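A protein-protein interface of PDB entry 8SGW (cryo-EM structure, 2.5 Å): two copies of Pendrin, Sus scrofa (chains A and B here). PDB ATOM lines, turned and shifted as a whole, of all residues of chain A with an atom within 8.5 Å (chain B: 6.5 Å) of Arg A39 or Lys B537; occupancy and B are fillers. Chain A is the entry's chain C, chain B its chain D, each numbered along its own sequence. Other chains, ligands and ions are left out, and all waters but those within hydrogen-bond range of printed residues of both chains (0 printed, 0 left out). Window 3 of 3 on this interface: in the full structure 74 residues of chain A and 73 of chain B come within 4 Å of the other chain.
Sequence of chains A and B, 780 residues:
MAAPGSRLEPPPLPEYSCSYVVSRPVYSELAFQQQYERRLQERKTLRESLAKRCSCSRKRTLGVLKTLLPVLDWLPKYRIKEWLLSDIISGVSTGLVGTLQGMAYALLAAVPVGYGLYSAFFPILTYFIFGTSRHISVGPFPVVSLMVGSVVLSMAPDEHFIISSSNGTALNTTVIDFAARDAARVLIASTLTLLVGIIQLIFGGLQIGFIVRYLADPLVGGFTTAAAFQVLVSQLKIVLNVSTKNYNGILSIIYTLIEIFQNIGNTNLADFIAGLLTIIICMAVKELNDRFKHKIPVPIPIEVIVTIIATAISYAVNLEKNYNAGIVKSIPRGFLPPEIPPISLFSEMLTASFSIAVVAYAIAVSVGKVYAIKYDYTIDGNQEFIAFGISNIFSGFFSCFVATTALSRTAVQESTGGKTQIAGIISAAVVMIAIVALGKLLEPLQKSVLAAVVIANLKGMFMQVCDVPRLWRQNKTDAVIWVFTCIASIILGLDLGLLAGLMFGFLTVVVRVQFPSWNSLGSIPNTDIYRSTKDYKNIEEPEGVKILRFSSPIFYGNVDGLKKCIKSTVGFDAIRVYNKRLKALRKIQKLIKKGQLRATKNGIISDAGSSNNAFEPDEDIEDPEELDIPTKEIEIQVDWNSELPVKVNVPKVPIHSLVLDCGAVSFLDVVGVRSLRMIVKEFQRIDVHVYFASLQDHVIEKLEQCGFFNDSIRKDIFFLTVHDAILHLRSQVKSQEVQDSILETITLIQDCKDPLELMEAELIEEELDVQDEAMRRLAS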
ATOM      1  N   GLN A  33      -3.212   6.447   1.852  1.00  0.00           N
ATOM      2  CA  GLN A  33      -3.082   5.098   1.315  1.00  0.00           C
ATOM      3  C   GLN A  33      -1.740   4.894   0.626  1.00  0.00           C
ATOM      4  O   GLN A  33      -1.182   3.792   0.674  1.00  0.00           O
ATOM      5  CB  GLN A  33      -4.228   4.808   0.348  1.00  0.00           C
ATOM      6  CG  GLN A  33      -5.582   4.702   1.023  1.00  0.00           C
ATOM      7  CD  GLN A  33      -5.648   3.553   2.006  1.00  0.00           C
ATOM      8  OE1 GLN A  33      -5.168   2.455   1.728  1.00  0.00           O
ATOM      9  NE2 GLN A  33      -6.239   3.803   3.169  1.00  0.00           N
ATOM     10  N   TYR A  36       0.883   5.014   3.949  1.00  0.00           N
ATOM     11  CA  TYR A  36       0.548   3.966   4.912  1.00  0.00           C
ATOM     12  C   TYR A  36      -0.233   2.882   4.181  1.00  0.00           C
ATOM     13  O   TYR A  36      -1.404   3.064   3.839  1.00  0.00           O
ATOM     14  CB  TYR A  36      -0.243   4.540   6.081  1.00  0.00           C
ATOM     15  CG  TYR A  36       0.538   5.527   6.919  1.00  0.00           C
ATOM     16  CD1 TYR A  36       1.607   5.110   7.700  1.00  0.00           C
ATOM     17  CD2 TYR A  36       0.210   6.875   6.922  1.00  0.00           C
ATOM     18  CE1 TYR A  36       2.324   6.009   8.465  1.00  0.00           C
ATOM     19  CE2 TYR A  36       0.921   7.781   7.684  1.00  0.00           C
ATOM     20  CZ  TYR A  36       1.977   7.343   8.453  1.00  0.00           C
ATOM     21  OH  TYR A  36       2.689   8.241   9.214  1.00  0.00           O
ATOM     22  N   GLU A  37       0.417   1.747   3.944  1.00  0.00           N
ATOM     23  CA  GLU A  37      -0.226   0.650   3.234  1.00  0.00           C
ATOM     24  C   GLU A  37      -1.275  -0.018   4.114  1.00  0.00           C
ATOM     25  O   GLU A  37      -1.122  -0.106   5.336  1.00  0.00           O
ATOM     26  CB  GLU A  37       0.820  -0.368   2.778  1.00  0.00           C
ATOM     27  CG  GLU A  37       1.474  -1.153   3.906  1.00  0.00           C
ATOM     28  CD  GLU A  37       2.648  -0.418   4.530  1.00  0.00           C
ATOM     29  OE1 GLU A  37       2.780   0.804   4.306  1.00  0.00           O
ATOM     30  OE2 GLU A  37       3.441  -1.065   5.246  1.00  0.00           O
ATOM     31  N   ARG A  38      -2.353  -0.476   3.487  1.00  0.00           N
ATOM     32  CA  ARG A  38      -3.423  -1.159   4.195  1.00  0.00           C
ATOM     33  C   ARG A  38      -3.174  -2.667   4.174  1.00  0.00           C
ATOM     34  O   ARG A  38      -2.103  -3.138   3.785  1.00  0.00           O
ATOM     35  CB  ARG A  38      -4.778  -0.801   3.588  1.00  0.00           C
ATOM     36  CG  ARG A  38      -5.429   0.422   4.208  1.00  0.00           C
ATOM     37  CD  ARG A  38      -6.876   0.572   3.764  1.00  0.00           C
ATOM     38  NE  ARG A  38      -7.795  -0.176   4.614  1.00  0.00           N
ATOM     39  CZ  ARG A  38      -9.115  -0.052   4.580  1.00  0.00           C
ATOM     40  NH1 ARG A  38      -9.709   0.779   3.739  1.00  0.00           N
ATOM     41  NH2 ARG A  38      -9.857  -0.780   5.409  1.00  0.00           N
ATOM     42  N   ARG A  39      -4.175  -3.434   4.605  1.00  0.00           N
ATOM     43  CA  ARG A  39      -4.119  -4.895   4.624  1.00  0.00           C
ATOM     44  C   ARG A  39      -2.921  -5.411   5.415  1.00  0.00           C
ATOM     45  O   ARG A  39      -3.076  -6.178   6.365  1.00  0.00           O
ATOM     46  CB  ARG A  39      -4.086  -5.448   3.197  1.00  0.00           C
ATOM     47  CG  ARG A  39      -5.396  -5.283   2.444  1.00  0.00           C
ATOM     48  CD  ARG A  39      -6.422  -6.313   2.883  1.00  0.00           C
ATOM     49  NE  ARG A  39      -7.668  -6.196   2.135  1.00  0.00           N
ATOM     50  CZ  ARG A  39      -8.736  -6.953   2.338  1.00  0.00           C
ATOM     51  NH1 ARG A  39      -8.749  -7.897   3.266  1.00  0.00           N
ATOM     52  NH2 ARG A  39      -9.822  -6.759   1.593  1.00  0.00           N
ATOM     53  N   GLU A 701     -14.667   2.213   1.018  1.00  0.00           N
ATOM     54  CA  GLU A 701     -14.743   0.975   0.249  1.00  0.00           C
ATOM     55  C   GLU A 701     -16.094   0.841  -0.447  1.00  0.00           C
ATOM     56  O   GLU A 701     -16.171   0.400  -1.601  1.00  0.00           O
ATOM     57  CB  GLU A 701     -14.484  -0.224   1.160  1.00  0.00           C
ATOM     58  CG  GLU A 701     -14.015  -1.468   0.429  1.00  0.00           C
ATOM     59  CD  GLU A 701     -13.671  -2.601   1.373  1.00  0.00           C
ATOM     60  OE1 GLU A 701     -13.970  -2.482   2.579  1.00  0.00           O
ATOM     61  OE2 GLU A 701     -13.099  -3.609   0.909  1.00  0.00           O
ATOM     62  N   GLU A 704     -15.988   3.120  -3.443  1.00  0.00           N
ATOM     63  CA  GLU A 704     -15.169   2.653  -4.557  1.00  0.00           C
ATOM     64  C   GLU A 704     -15.791   1.447  -5.249  1.00  0.00           C
ATOM     65  O   GLU A 704     -15.613   1.279  -6.460  1.00  0.00           O
ATOM     66  CB  GLU A 704     -13.748   2.330  -4.091  1.00  0.00           C
ATOM     67  CG  GLU A 704     -13.623   1.133  -3.172  1.00  0.00           C
ATOM     68  CD  GLU A 704     -12.202   0.910  -2.696  1.00  0.00           C
ATOM     69  OE1 GLU A 704     -11.318   1.709  -3.066  1.00  0.00           O
ATOM     70  OE2 GLU A 704     -11.969  -0.066  -1.953  1.00  0.00           O
ATOM     71  N   SER B 532      -7.922   1.017  12.691  1.00  0.00           N
ATOM     72  CA  SER B 532      -8.036  -0.355  13.171  1.00  0.00           C
ATOM     73  C   SER B 532      -6.695  -1.072  13.075  1.00  0.00           C
ATOM     74  O   SER B 532      -6.007  -1.000  12.053  1.00  0.00           O
ATOM     75  CB  SER B 532      -9.103  -1.102  12.375  1.00  0.00           C
ATOM     76  OG  SER B 532      -8.957  -0.864  10.989  1.00  0.00           O
ATOM     77  N   THR B 533      -6.328  -1.769  14.154  1.00  0.00           N
ATOM     78  CA  THR B 533      -5.018  -2.401  14.242  1.00  0.00           C
ATOM     79  C   THR B 533      -4.845  -3.541  13.247  1.00  0.00           C
ATOM     80  O   THR B 533      -3.709  -3.913  12.942  1.00  0.00           O
ATOM     81  CB  THR B 533      -4.784  -2.925  15.659  1.00  0.00           C
ATOM     82  OG1 THR B 533      -5.863  -3.789  16.032  1.00  0.00           O
ATOM     83  CG2 THR B 533      -4.716  -1.774  16.647  1.00  0.00           C
ATOM     84  N   LYS B 534      -5.938  -4.100  12.740  1.00  0.00           N
ATOM     85  CA  LYS B 534      -5.889  -5.244  11.843  1.00  0.00           C
ATOM     86  C   LYS B 534      -5.883  -4.854  10.371  1.00  0.00           C
ATOM     87  O   LYS B 534      -5.863  -5.742   9.513  1.00  0.00           O
ATOM     88  CB  LYS B 534      -7.076  -6.171  12.118  1.00  0.00           C
ATOM     89  CG  LYS B 534      -8.424  -5.473  12.026  1.00  0.00           C
ATOM     90  CD  LYS B 534      -9.572  -6.429  12.296  1.00  0.00           C
ATOM     91  CE  LYS B 534     -10.895  -5.687  12.355  1.00  0.00           C
ATOM     92  NZ  LYS B 534     -11.194  -4.989  11.075  1.00  0.00           N
ATOM     93  N   ASP B 535      -5.894  -3.560  10.057  1.00  0.00           N
ATOM     94  CA  ASP B 535      -6.060  -3.107   8.683  1.00  0.00           C
ATOM     95  C   ASP B 535      -4.813  -2.494   8.067  1.00  0.00           C
ATOM     96  O   ASP B 535      -4.648  -2.576   6.850  1.00  0.00           O
ATOM     97  CB  ASP B 535      -7.199  -2.084   8.595  1.00  0.00           C
ATOM     98  CG  ASP B 535      -8.567  -2.731   8.636  1.00  0.00           C
ATOM     99  OD1 ASP B 535      -8.668  -3.879   9.116  1.00  0.00           O
ATOM    100  OD2 ASP B 535      -9.544  -2.091   8.194  1.00  0.00           O
ATOM    101  N   TYR B 536      -3.932  -1.882   8.860  1.00  0.00           N
ATOM    102  CA  TYR B 536      -2.836  -1.108   8.297  1.00  0.00           C
ATOM    103  C   TYR B 536      -1.453  -1.700   8.537  1.00  0.00           C
ATOM    104  O   TYR B 536      -0.525  -1.361   7.799  1.00  0.00           O
ATOM    105  CB  TYR B 536      -2.869   0.327   8.844  1.00  0.00           C
ATOM    106  CG  TYR B 536      -4.004   1.150   8.277  1.00  0.00           C
ATOM    107  CD1 TYR B 536      -5.308   0.968   8.717  1.00  0.00           C
ATOM    108  CD2 TYR B 536      -3.776   2.098   7.290  1.00  0.00           C
ATOM    109  CE1 TYR B 536      -6.349   1.710   8.198  1.00  0.00           C
ATOM    110  CE2 TYR B 536      -4.811   2.846   6.764  1.00  0.00           C
ATOM    111  CZ  TYR B 536      -6.094   2.648   7.222  1.00  0.00           C
ATOM    112  OH  TYR B 536      -7.127   3.390   6.702  1.00  0.00           O
ATOM    113  N   LYS B 537      -1.289  -2.550   9.551  1.00  0.00           N
ATOM    114  CA  LYS B 537      -0.063  -3.281   9.871  1.00  0.00           C
ATOM    115  C   LYS B 537       1.068  -2.380  10.355  1.00  0.00           C
ATOM    116  O   LYS B 537       2.124  -2.893  10.741  1.00  0.00           O
ATOM    117  CB  LYS B 537       0.448  -4.120   8.689  1.00  0.00           C
ATOM    118  CG  LYS B 537      -0.560  -5.125   8.161  1.00  0.00           C
ATOM    119  CD  LYS B 537      -0.818  -6.236   9.165  1.00  0.00           C
ATOM    120  CE  LYS B 537      -2.260  -6.224   9.646  1.00  0.00           C
ATOM    121  NZ  LYS B 537      -2.580  -7.420  10.470  1.00  0.00           N
ATOM    122  N   ASN B 538       0.887  -1.060  10.350  1.00  0.00           N
ATOM    123  CA  ASN B 538       1.829  -0.136  10.970  1.00  0.00           C
ATOM    124  C   ASN B 538       1.227   0.528  12.198  1.00  0.00           C
ATOM    125  O   ASN B 538       1.767   1.529  12.684  1.00  0.00           O
ATOM    126  CB  ASN B 538       2.288   0.925   9.965  1.00  0.00           C
ATOM    127  CG  ASN B 538       3.698   1.412  10.237  1.00  0.00           C
ATOM    128  OD1 ASN B 538       4.549   0.656  10.706  1.00  0.00           O
ATOM    129  ND2 ASN B 538       3.952   2.682   9.944  1.00  0.00           N
ATOM    130  N   ILE B 539       0.124  -0.008  12.708  1.00  0.00           N
ATOM    131  CA  ILE B 539      -0.601   0.582  13.823  1.00  0.00           C
ATOM    132  C   ILE B 539      -0.055   0.007  15.121  1.00  0.00           C
ATOM    133  O   ILE B 539       0.048  -1.216  15.276  1.00  0.00           O
ATOM    134  CB  ILE B 539      -2.108   0.313  13.690  1.00  0.00           C
ATOM    135  CG1 ILE B 539      -2.675   1.027  12.461  1.00  0.00           C
ATOM    136  CG2 ILE B 539      -2.831   0.741  14.939  1.00  0.00           C
ATOM    137  CD1 ILE B 539      -3.049   2.466  12.707  1.00  0.00           C
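O of Glu A37 lies close to O of Tyr B536 (2.8 Å).
The backbone NH (N) of Arg A39 sits at hydrogen-bond distance from the backbone carbonyl oxygen (O) of Asp B535.
The guanidinium group of Arg A38 lies within salt-bridge range of the side-chain carboxylate of Asp B535, 3.1 Å away.
The side-chain hydroxyl (OG) of Ser B532 sits close to the side-chain carboxylate (OD2) of Asp B535 (3.1 Å).
The side-chain amino group (NZ) of Lys B534 is in salt-bridge range of the side-chain carboxylate (OD1) of Asp B535.
Among the printed residues, pairs that only touch across the chains: Gln A33 with Tyr B536 (3.7 Å), Tyr A36 with Asn B538 (3.99 Å), Arg A38 with Tyr B536 (3.6 Å) and Arg A39 with Lys B537 (3.3 Å).
Of chain A, only Arg A39 (3.3 Å) comes within 4 Å of Lys B537.
Of the printed residues of chain B, Glu A37 touches Tyr B536.
Of the printed residues of chain A, Tyr B536 touches Gln A33, Glu A37 and Arg A38.
Printed residues of chain B within 4 Å of Arg A38: Asp B535 (3.1 Å) and Tyr B536 (3.6 Å).
Ile B539 touches none of the printed residues of chain A.
The nearest residue of chain A that does not touch Lys B537 is Glu A37 (4.9 Å).
Printed residues of chain B that touch a printed residue of chain A: Asp B535, Tyr B536, Lys B537 and Asn B538.
Hydrophobic or aromatic side chains of chain B that line the printed part of chain A: Tyr B536.
Along chain B the printed residues that touch a printed residue of chain A span positions 535 to 538.
Of the 7 printed residues of chain A, 5 touch a printed residue of chain B.
Along chain A the printed residues that touch a printed residue of chain B span positions 33 to 39.
No position is printed for both chains.
Of the 7 pairs that touch across the chains among the printed residues, none has its exchanged pair printed and touching as well.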
